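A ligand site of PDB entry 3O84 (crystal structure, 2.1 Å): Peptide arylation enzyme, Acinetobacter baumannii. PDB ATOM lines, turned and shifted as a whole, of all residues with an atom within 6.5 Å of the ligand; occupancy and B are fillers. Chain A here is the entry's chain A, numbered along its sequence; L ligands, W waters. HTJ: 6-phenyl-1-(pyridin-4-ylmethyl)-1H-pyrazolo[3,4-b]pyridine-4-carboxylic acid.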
ATOM      1  N   GLY A 200     -15.534 -16.662 -12.607  1.00  0.00           N
ATOM      2  CA  GLY A 200     -15.125 -17.137 -11.282  1.00  0.00           C
ATOM      3  C   GLY A 200     -16.217 -17.982 -10.646  1.00  0.00           C
ATOM      4  O   GLY A 200     -17.373 -17.968 -11.106  1.00  0.00           O
ATOM      5  N   LEU A 239      -3.267  -9.685  -4.679  1.00  0.00           N
ATOM      6  CA  LEU A 239      -4.169 -10.682  -5.293  1.00  0.00           C
ATOM      7  C   LEU A 239      -3.606 -11.037  -6.677  1.00  0.00           C
ATOM      8  O   LEU A 239      -2.707 -10.350  -7.171  1.00  0.00           O
ATOM      9  CB  LEU A 239      -5.599 -10.137  -5.388  1.00  0.00           C
ATOM     10  CG  LEU A 239      -6.319  -9.732  -4.107  1.00  0.00           C
ATOM     11  CD1 LEU A 239      -7.660  -9.078  -4.436  1.00  0.00           C
ATOM     12  CD2 LEU A 239      -6.495 -10.926  -3.150  1.00  0.00           C
ATOM     13  N   PRO A 240      -4.104 -12.127  -7.309  1.00  0.00           N
ATOM     14  CA  PRO A 240      -3.572 -12.499  -8.625  1.00  0.00           C
ATOM     15  C   PRO A 240      -3.763 -11.366  -9.644  1.00  0.00           C
ATOM     16  O   PRO A 240      -4.887 -10.882  -9.857  1.00  0.00           O
ATOM     17  CB  PRO A 240      -4.402 -13.731  -9.003  1.00  0.00           C
ATOM     18  CG  PRO A 240      -4.825 -14.319  -7.658  1.00  0.00           C
ATOM     19  CD  PRO A 240      -5.117 -13.096  -6.826  1.00  0.00           C
ATOM     20  N   HIS A 243      -6.724 -11.294 -12.246  1.00  0.00           N
ATOM     21  CA  HIS A 243      -8.104 -11.272 -11.764  1.00  0.00           C
ATOM     22  C   HIS A 243      -8.741  -9.896 -11.995  1.00  0.00           C
ATOM     23  O   HIS A 243      -8.110  -8.872 -11.752  1.00  0.00           O
ATOM     24  CB  HIS A 243      -8.209 -11.675 -10.281  1.00  0.00           C
ATOM     25  CG  HIS A 243      -9.610 -12.008  -9.862  1.00  0.00           C
ATOM     26  ND1 HIS A 243     -10.570 -11.038  -9.651  1.00  0.00           N
ATOM     27  CD2 HIS A 243     -10.231 -13.188  -9.670  1.00  0.00           C
ATOM     28  CE1 HIS A 243     -11.721 -11.611  -9.333  1.00  0.00           C
ATOM     29  NE2 HIS A 243     -11.542 -12.925  -9.341  1.00  0.00           N
ATOM     30  N   ASN A 244      -9.979  -9.903 -12.467  1.00  0.00           N
ATOM     31  CA  ASN A 244     -10.718  -8.665 -12.764  1.00  0.00           C
ATOM     32  C   ASN A 244     -10.611  -7.614 -11.657  1.00  0.00           C
ATOM     33  O   ASN A 244     -10.471  -6.414 -11.921  1.00  0.00           O
ATOM     34  CB  ASN A 244     -12.192  -8.985 -13.034  1.00  0.00           C
ATOM     35  CG  ASN A 244     -12.889  -7.906 -13.885  1.00  0.00           C
ATOM     36  OD1 ASN A 244     -12.446  -7.585 -14.988  1.00  0.00           O
ATOM     37  ND2 ASN A 244     -13.982  -7.349 -13.349  1.00  0.00           N
ATOM     38  N   PHE A 245     -10.674  -8.084 -10.400  1.00  0.00           N
ATOM     39  CA  PHE A 245     -10.605  -7.246  -9.205  1.00  0.00           C
ATOM     40  C   PHE A 245      -9.250  -6.547  -9.162  1.00  0.00           C
ATOM     41  O   PHE A 245      -9.184  -5.309  -9.059  1.00  0.00           O
ATOM     42  CB  PHE A 245     -10.861  -8.104  -7.954  1.00  0.00           C
ATOM     43  CG  PHE A 245     -10.958  -7.338  -6.643  1.00  0.00           C
ATOM     44  CD1 PHE A 245     -11.262  -5.968  -6.613  1.00  0.00           C
ATOM     45  CD2 PHE A 245     -10.796  -8.003  -5.434  1.00  0.00           C
ATOM     46  CE1 PHE A 245     -11.366  -5.268  -5.397  1.00  0.00           C
ATOM     47  CE2 PHE A 245     -10.892  -7.334  -4.200  1.00  0.00           C
ATOM     48  CZ  PHE A 245     -11.186  -5.952  -4.175  1.00  0.00           C
ATOM     49  N   MET A 246      -8.174  -7.334  -9.264  1.00  0.00           N
ATOM     50  CA  MET A 246      -6.822  -6.786  -9.180  1.00  0.00           C
ATOM     51  C   MET A 246      -6.383  -6.021 -10.456  1.00  0.00           C
ATOM     52  O   MET A 246      -5.450  -5.205 -10.418  1.00  0.00           O
ATOM     53  CB  MET A 246      -5.821  -7.897  -8.872  1.00  0.00           C
ATOM     54  CG  MET A 246      -4.511  -7.411  -8.257  1.00  0.00           C
ATOM     55  SD  MET A 246      -4.734  -6.742  -6.588  1.00  0.00           S
ATOM     56  CE  MET A 246      -4.814  -4.949  -6.853  1.00  0.00           C
ATOM     57  N   SER A 248      -8.703  -4.338 -12.822  1.00  0.00           N
ATOM     58  CA  SER A 248      -9.570  -3.277 -13.335  1.00  0.00           C
ATOM     59  C   SER A 248     -10.498  -2.586 -12.326  1.00  0.00           C
ATOM     60  O   SER A 248     -11.235  -1.667 -12.724  1.00  0.00           O
ATOM     61  CB  SER A 248     -10.418  -3.849 -14.479  1.00  0.00           C
ATOM     62  OG  SER A 248     -11.413  -4.725 -13.986  1.00  0.00           O
ATOM     63  N   SER A 249     -10.464  -2.992 -11.059  1.00  0.00           N
ATOM     64  CA  SER A 249     -11.506  -2.568 -10.120  1.00  0.00           C
ATOM     65  C   SER A 249     -11.070  -1.901  -8.815  1.00  0.00           C
ATOM     66  O   SER A 249     -11.425  -2.384  -7.738  1.00  0.00           O
ATOM     67  CB  SER A 249     -12.438  -3.753  -9.810  1.00  0.00           C
ATOM     68  OG  SER A 249     -13.001  -4.257 -11.012  1.00  0.00           O
ATOM     69  N   VAL A 288      -9.433 -10.034  -0.456  1.00  0.00           N
ATOM     70  CA  VAL A 288     -10.623 -10.830  -0.175  1.00  0.00           C
ATOM     71  C   VAL A 288     -10.686 -11.087   1.366  1.00  0.00           C
ATOM     72  O   VAL A 288      -9.659 -10.988   2.037  1.00  0.00           O
ATOM     73  CB  VAL A 288     -10.592 -12.168  -0.968  1.00  0.00           C
ATOM     74  CG1 VAL A 288     -10.467 -11.888  -2.474  1.00  0.00           C
ATOM     75  CG2 VAL A 288      -9.431 -13.068  -0.504  1.00  0.00           C
ATOM     76  N   VAL A 314     -12.197  -4.457  -0.156  1.00  0.00           N
ATOM     77  CA  VAL A 314     -12.473  -5.830   0.200  1.00  0.00           C
ATOM     78  C   VAL A 314     -13.606  -6.345  -0.675  1.00  0.00           C
ATOM     79  O   VAL A 314     -14.702  -5.782  -0.707  1.00  0.00           O
ATOM     80  CB  VAL A 314     -12.810  -6.011   1.723  1.00  0.00           C
ATOM     81  CG1 VAL A 314     -13.045  -7.498   2.029  1.00  0.00           C
ATOM     82  CG2 VAL A 314     -11.692  -5.445   2.609  1.00  0.00           C
ATOM     83  N   GLY A 315     -13.331  -7.419  -1.395  1.00  0.00           N
ATOM     84  CA  GLY A 315     -14.361  -8.018  -2.228  1.00  0.00           C
ATOM     85  C   GLY A 315     -14.327  -9.512  -2.103  1.00  0.00           C
ATOM     86  O   GLY A 315     -13.301 -10.099  -1.764  1.00  0.00           O
ATOM     87  N   GLY A 316     -15.456 -10.136  -2.379  1.00  0.00           N
ATOM     88  CA  GLY A 316     -15.457 -11.560  -2.520  1.00  0.00           C
ATOM     89  C   GLY A 316     -16.561 -12.205  -1.739  1.00  0.00           C
ATOM     90  O   GLY A 316     -17.751 -11.896  -1.945  1.00  0.00           O
ATOM     91  N   ALA A 317     -16.127 -13.067  -0.831  1.00  0.00           N
ATOM     92  CA  ALA A 317     -16.930 -14.055  -0.130  1.00  0.00           C
ATOM     93  C   ALA A 317     -18.006 -13.437   0.753  1.00  0.00           C
ATOM     94  O   ALA A 317     -18.997 -12.899   0.273  1.00  0.00           O
ATOM     95  CB  ALA A 317     -15.988 -14.958   0.699  1.00  0.00           C
ATOM     96  N   VAL A 338     -16.380  -4.040  -2.289  1.00  0.00           N
ATOM     97  CA  VAL A 338     -16.501  -4.177  -3.728  1.00  0.00           C
ATOM     98  C   VAL A 338     -17.198  -5.498  -4.032  1.00  0.00           C
ATOM     99  O   VAL A 338     -16.763  -6.551  -3.551  1.00  0.00           O
ATOM    100  CB  VAL A 338     -15.116  -4.118  -4.437  1.00  0.00           C
ATOM    101  CG1 VAL A 338     -15.294  -4.101  -5.962  1.00  0.00           C
ATOM    102  CG2 VAL A 338     -14.308  -2.922  -3.977  1.00  0.00           C
ATOM    103  N   PHE A 339     -18.262  -5.445  -4.812  1.00  0.00           N
ATOM    104  CA  PHE A 339     -18.862  -6.675  -5.313  1.00  0.00           C
ATOM    105  C   PHE A 339     -18.956  -6.605  -6.822  1.00  0.00           C
ATOM    106  O   PHE A 339     -19.714  -5.802  -7.372  1.00  0.00           O
ATOM    107  CB  PHE A 339     -20.256  -6.943  -4.722  1.00  0.00           C
ATOM    108  CG  PHE A 339     -20.923  -8.123  -5.367  1.00  0.00           C
ATOM    109  CD1 PHE A 339     -20.469  -9.406  -5.133  1.00  0.00           C
ATOM    110  CD2 PHE A 339     -21.976  -7.935  -6.250  1.00  0.00           C
ATOM    111  CE1 PHE A 339     -21.068 -10.501  -5.759  1.00  0.00           C
ATOM    112  CE2 PHE A 339     -22.585  -9.020  -6.872  1.00  0.00           C
ATOM    113  CZ  PHE A 339     -22.120 -10.295  -6.634  1.00  0.00           C
ATOM    114  N   GLY A 340     -18.178  -7.437  -7.494  1.00  0.00           N
ATOM    115  CA  GLY A 340     -18.125  -7.419  -8.945  1.00  0.00           C
ATOM    116  C   GLY A 340     -18.076  -8.796  -9.536  1.00  0.00           C
ATOM    117  O   GLY A 340     -18.157  -9.801  -8.819  1.00  0.00           O
ATOM    118  N   MET A 341     -17.958  -8.851 -10.864  1.00  0.00           N
ATOM    119  CA  MET A 341     -17.838 -10.096 -11.590  1.00  0.00           C
ATOM    120  C   MET A 341     -17.031  -9.829 -12.860  1.00  0.00           C
ATOM    121  O   MET A 341     -17.152  -8.740 -13.458  1.00  0.00           O
ATOM    122  CB  MET A 341     -19.214 -10.665 -11.937  1.00  0.00           C
ATOM    123  CG  MET A 341     -20.110  -9.700 -12.693  1.00  0.00           C
ATOM    124  SD  MET A 341     -21.862 -10.121 -12.688  1.00  0.00           S
ATOM    125  CE  MET A 341     -22.280  -9.740 -10.980  1.00  0.00           C
ATOM    126  N   ALA A 342     -16.212 -10.793 -13.249  1.00  0.00           N
ATOM    127  CA  ALA A 342     -15.438 -10.693 -14.486  1.00  0.00           C
ATOM    128  C   ALA A 342     -16.337 -10.546 -15.723  1.00  0.00           C
ATOM    129  O   ALA A 342     -15.879 -10.048 -16.757  1.00  0.00           O
ATOM    130  CB  ALA A 342     -14.497 -11.883 -14.623  1.00  0.00           C
ATOM    131  N   GLY A 344     -18.748  -8.436 -15.964  1.00  0.00           N
ATOM    132  CA  GLY A 344     -19.029  -7.017 -16.142  1.00  0.00           C
ATOM    133  C   GLY A 344     -19.246  -6.238 -14.862  1.00  0.00           C
ATOM    134  O   GLY A 344     -18.278  -5.763 -14.252  1.00  0.00           O
ATOM    135  N   LEU A 345     -20.508  -6.120 -14.465  1.00  0.00           N
ATOM    136  CA  LEU A 345     -20.945  -5.331 -13.307  1.00  0.00           C
ATOM    137  C   LEU A 345     -20.006  -5.354 -12.112  1.00  0.00           C
ATOM    138  O   LEU A 345     -19.673  -6.423 -11.597  1.00  0.00           O
ATOM    139  CB  LEU A 345     -22.338  -5.802 -12.852  1.00  0.00           C
ATOM    140  CG  LEU A 345     -22.921  -5.088 -11.624  1.00  0.00           C
ATOM    141  CD1 LEU A 345     -23.220  -3.619 -11.956  1.00  0.00           C
ATOM    142  CD2 LEU A 345     -24.193  -5.801 -11.121  1.00  0.00           C
ATOM    143  N   VAL A 346     -19.581  -4.157 -11.697  1.00  0.00           N
ATOM    144  CA  VAL A 346     -18.865  -3.975 -10.449  1.00  0.00           C
ATOM    145  C   VAL A 346     -19.571  -2.905  -9.612  1.00  0.00           C
ATOM    146  O   VAL A 346     -19.956  -1.854 -10.125  1.00  0.00           O
ATOM    147  CB  VAL A 346     -17.394  -3.538 -10.675  1.00  0.00           C
ATOM    148  CG1 VAL A 346     -16.666  -3.456  -9.329  1.00  0.00           C
ATOM    149  CG2 VAL A 346     -16.658  -4.497 -11.614  1.00  0.00           C
ATOM    150  N   ASN A 347     -19.739  -3.207  -8.316  1.00  0.00           N
ATOM    151  CA  ASN A 347     -20.329  -2.307  -7.322  1.00  0.00           C
ATOM    152  C   ASN A 347     -19.282  -1.883  -6.304  1.00  0.00           C
ATOM    153  O   ASN A 347     -18.487  -2.707  -5.861  1.00  0.00           O
ATOM    154  CB  ASN A 347     -21.460  -3.029  -6.587  1.00  0.00           C
ATOM    155  CG  ASN A 347     -22.532  -3.534  -7.544  1.00  0.00           C
ATOM    156  OD1 ASN A 347     -23.446  -2.805  -7.902  1.00  0.00           O
ATOM    157  ND2 ASN A 347     -22.412  -4.799  -7.960  1.00  0.00           N
ATOM    158  N   TYR A 348     -19.291  -0.593  -5.939  1.00  0.00           N
ATOM    159  CA  TYR A 348     -18.405  -0.052  -4.928  1.00  0.00           C
ATOM    160  C   TYR A 348     -19.204   0.749  -3.920  1.00  0.00           C
ATOM    161  O   TYR A 348     -20.094   1.520  -4.302  1.00  0.00           O
ATOM    162  CB  TYR A 348     -17.430   0.952  -5.528  1.00  0.00           C
ATOM    163  CG  TYR A 348     -16.508   0.429  -6.615  1.00  0.00           C
ATOM    164  CD1 TYR A 348     -16.857   0.554  -7.954  1.00  0.00           C
ATOM    165  CD2 TYR A 348     -15.278  -0.122  -6.297  1.00  0.00           C
ATOM    166  CE1 TYR A 348     -15.997   0.120  -8.958  1.00  0.00           C
ATOM    167  CE2 TYR A 348     -14.409  -0.564  -7.283  1.00  0.00           C
ATOM    168  CZ  TYR A 348     -14.778  -0.442  -8.613  1.00  0.00           C
ATOM    169  OH  TYR A 348     -13.948  -0.872  -9.595  1.00  0.00           O
ATOM    170  N   ASP A 422     -26.263 -14.491  -8.431  1.00  0.00           N
ATOM    171  CA  ASP A 422     -26.150 -13.851  -7.126  1.00  0.00           C
ATOM    172  C   ASP A 422     -27.500 -13.480  -6.518  1.00  0.00           C
ATOM    173  O   ASP A 422     -28.385 -12.985  -7.213  1.00  0.00           O
ATOM    174  CB  ASP A 422     -25.242 -12.619  -7.197  1.00  0.00           C
ATOM    175  CG  ASP A 422     -23.839 -12.956  -7.623  1.00  0.00           C
ATOM    176  OD1 ASP A 422     -23.391 -12.454  -8.688  1.00  0.00           O
ATOM    177  OD2 ASP A 422     -23.168 -13.737  -6.912  1.00  0.00           O
ATOM    178  N   ARG A 437     -25.957 -17.069  -3.065  1.00  0.00           N
ATOM    179  CA  ARG A 437     -25.772 -17.503  -4.443  1.00  0.00           C
ATOM    180  C   ARG A 437     -26.696 -18.658  -4.778  1.00  0.00           C
ATOM    181  O   ARG A 437     -26.993 -19.492  -3.935  1.00  0.00           O
ATOM    182  CB  ARG A 437     -24.313 -17.914  -4.670  1.00  0.00           C
ATOM    183  CG  ARG A 437     -23.855 -17.732  -6.100  1.00  0.00           C
ATOM    184  CD  ARG A 437     -22.375 -18.012  -6.278  1.00  0.00           C
ATOM    185  NE  ARG A 437     -21.996 -17.943  -7.685  1.00  0.00           N
ATOM    186  CZ  ARG A 437     -20.914 -18.517  -8.207  1.00  0.00           C
ATOM    187  NH1 ARG A 437     -20.086 -19.219  -7.433  1.00  0.00           N
ATOM    188  NH2 ARG A 437     -20.660 -18.385  -9.512  1.00  0.00           N
HETATM  189  C1  HTJ L   1     -14.272  -6.904  -9.729  1.00  0.00           C
HETATM  190  C2  HTJ L   1     -14.359  -6.962  -8.329  1.00  0.00           C
HETATM  191  C3  HTJ L   1     -14.590  -8.190  -7.697  1.00  0.00           C
HETATM  192  C4  HTJ L   1     -14.732  -9.322  -8.523  1.00  0.00           C
HETATM  193  C5  HTJ L   1     -14.631  -9.211  -9.920  1.00  0.00           C
HETATM  194  N6  HTJ L   1     -14.421  -8.001 -10.484  1.00  0.00           N
HETATM  195  C7  HTJ L   1     -14.700  -8.295  -6.166  1.00  0.00           C
HETATM  196  N8  HTJ L   1     -15.331  -9.589  -5.917  1.00  0.00           N
HETATM  197  C9  HTJ L   1     -14.802 -10.808  -5.838  1.00  0.00           C
HETATM  198  C10 HTJ L   1     -15.888 -11.662  -5.690  1.00  0.00           C
HETATM  199  C11 HTJ L   1     -17.118 -10.915  -5.687  1.00  0.00           C
HETATM  200  N12 HTJ L   1     -16.738  -9.619  -5.844  1.00  0.00           N
HETATM  201  N13 HTJ L   1     -13.535 -11.249  -5.865  1.00  0.00           N
HETATM  202  C14 HTJ L   1     -13.244 -12.549  -5.754  1.00  0.00           C
HETATM  203  C15 HTJ L   1     -14.275 -13.475  -5.581  1.00  0.00           C
HETATM  204  C16 HTJ L   1     -15.612 -13.032  -5.544  1.00  0.00           C
HETATM  205  C18 HTJ L   1     -16.730 -14.026  -5.373  1.00  0.00           C
HETATM  206  O19 HTJ L   1     -16.473 -15.164  -4.936  1.00  0.00           O
HETATM  207  O20 HTJ L   1     -17.910 -13.721  -5.668  1.00  0.00           O
HETATM  208  C21 HTJ L   1     -11.801 -12.934  -5.794  1.00  0.00           C
HETATM  209  C22 HTJ L   1     -10.859 -11.982  -6.177  1.00  0.00           C
HETATM  210  C23 HTJ L   1      -9.503 -12.310  -6.227  1.00  0.00           C
HETATM  211  C24 HTJ L   1      -9.089 -13.604  -5.889  1.00  0.00           C
HETATM  212  C25 HTJ L   1     -10.022 -14.566  -5.510  1.00  0.00           C
HETATM  213  C26 HTJ L   1     -11.388 -14.228  -5.456  1.00  0.00           C
HETATM  214  O   HOH W   1     -18.558 -12.297  -8.394  1.00  0.00           O
HETATM  215  O   HOH W   2     -19.658 -16.218  -5.661  1.00  0.00           O
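ND2 of Asn 244 lies within hydrogen-bond range of N6 of the ligand (3.0 Å).
The backbone NH (N) of Gly 340 is in hydrogen-bond range of a nitrogen (N12) of the ligand, at 3.1 Å.
OG of Ser 249 is in hydrogen-bond range of O of Asn 244 (3.4 Å).
The backbone carbonyl oxygen (O) of Met 341 is in hydrogen-bond range of the side-chain amide nitrogen (ND2) of Asn 244 (3.5 Å).
OG of Ser 248 is in hydrogen-bond range of O of Asn 244 (2.8 Å).
The side-chain hydroxyl (OG) of Ser 248 lies close to the side-chain hydroxyl (OG) of Ser 249, 3.4 Å away.
The backbone carbonyl oxygen (O) of Ser 249 lies close to the side-chain hydroxyl (OH) of Tyr 348 (3.5 Å).
A ring nitrogen (ND1) of His 243 lies within hydrogen-bond range of the backbone NH (N) of Phe 245, 3.0 Å away.
The backbone NH (N) of Asn 347 sits at hydrogen-bond distance from the backbone carbonyl oxygen (O) of Phe 339 (2.8 Å).
The backbone carbonyl oxygen (O) of Val 314 sits at hydrogen-bond distance from the backbone NH (N) of Val 338.
Residues that only touch the ligand: His 243, Phe 245, Ser 249, Val 288, Gly 315, Gly 316, Val 338, Phe 339, Met 341 and Val 346.
Hydrophobic or aromatic side chains within 4 Å of the ligand: His 243, Phe 245, Val 288, Val 338, Phe 339 and Val 346.
Within 4 Å of the ligand: His 243, Asn 244, Phe 245, Ser 249, Val 288, Gly 315, Gly 316, Val 338, Phe 339, Gly 340, Met 341 and Val 346.
Water W1 bridges O of Gly 340 (2.6 Å) and O20 of the ligand (3.1 Å).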
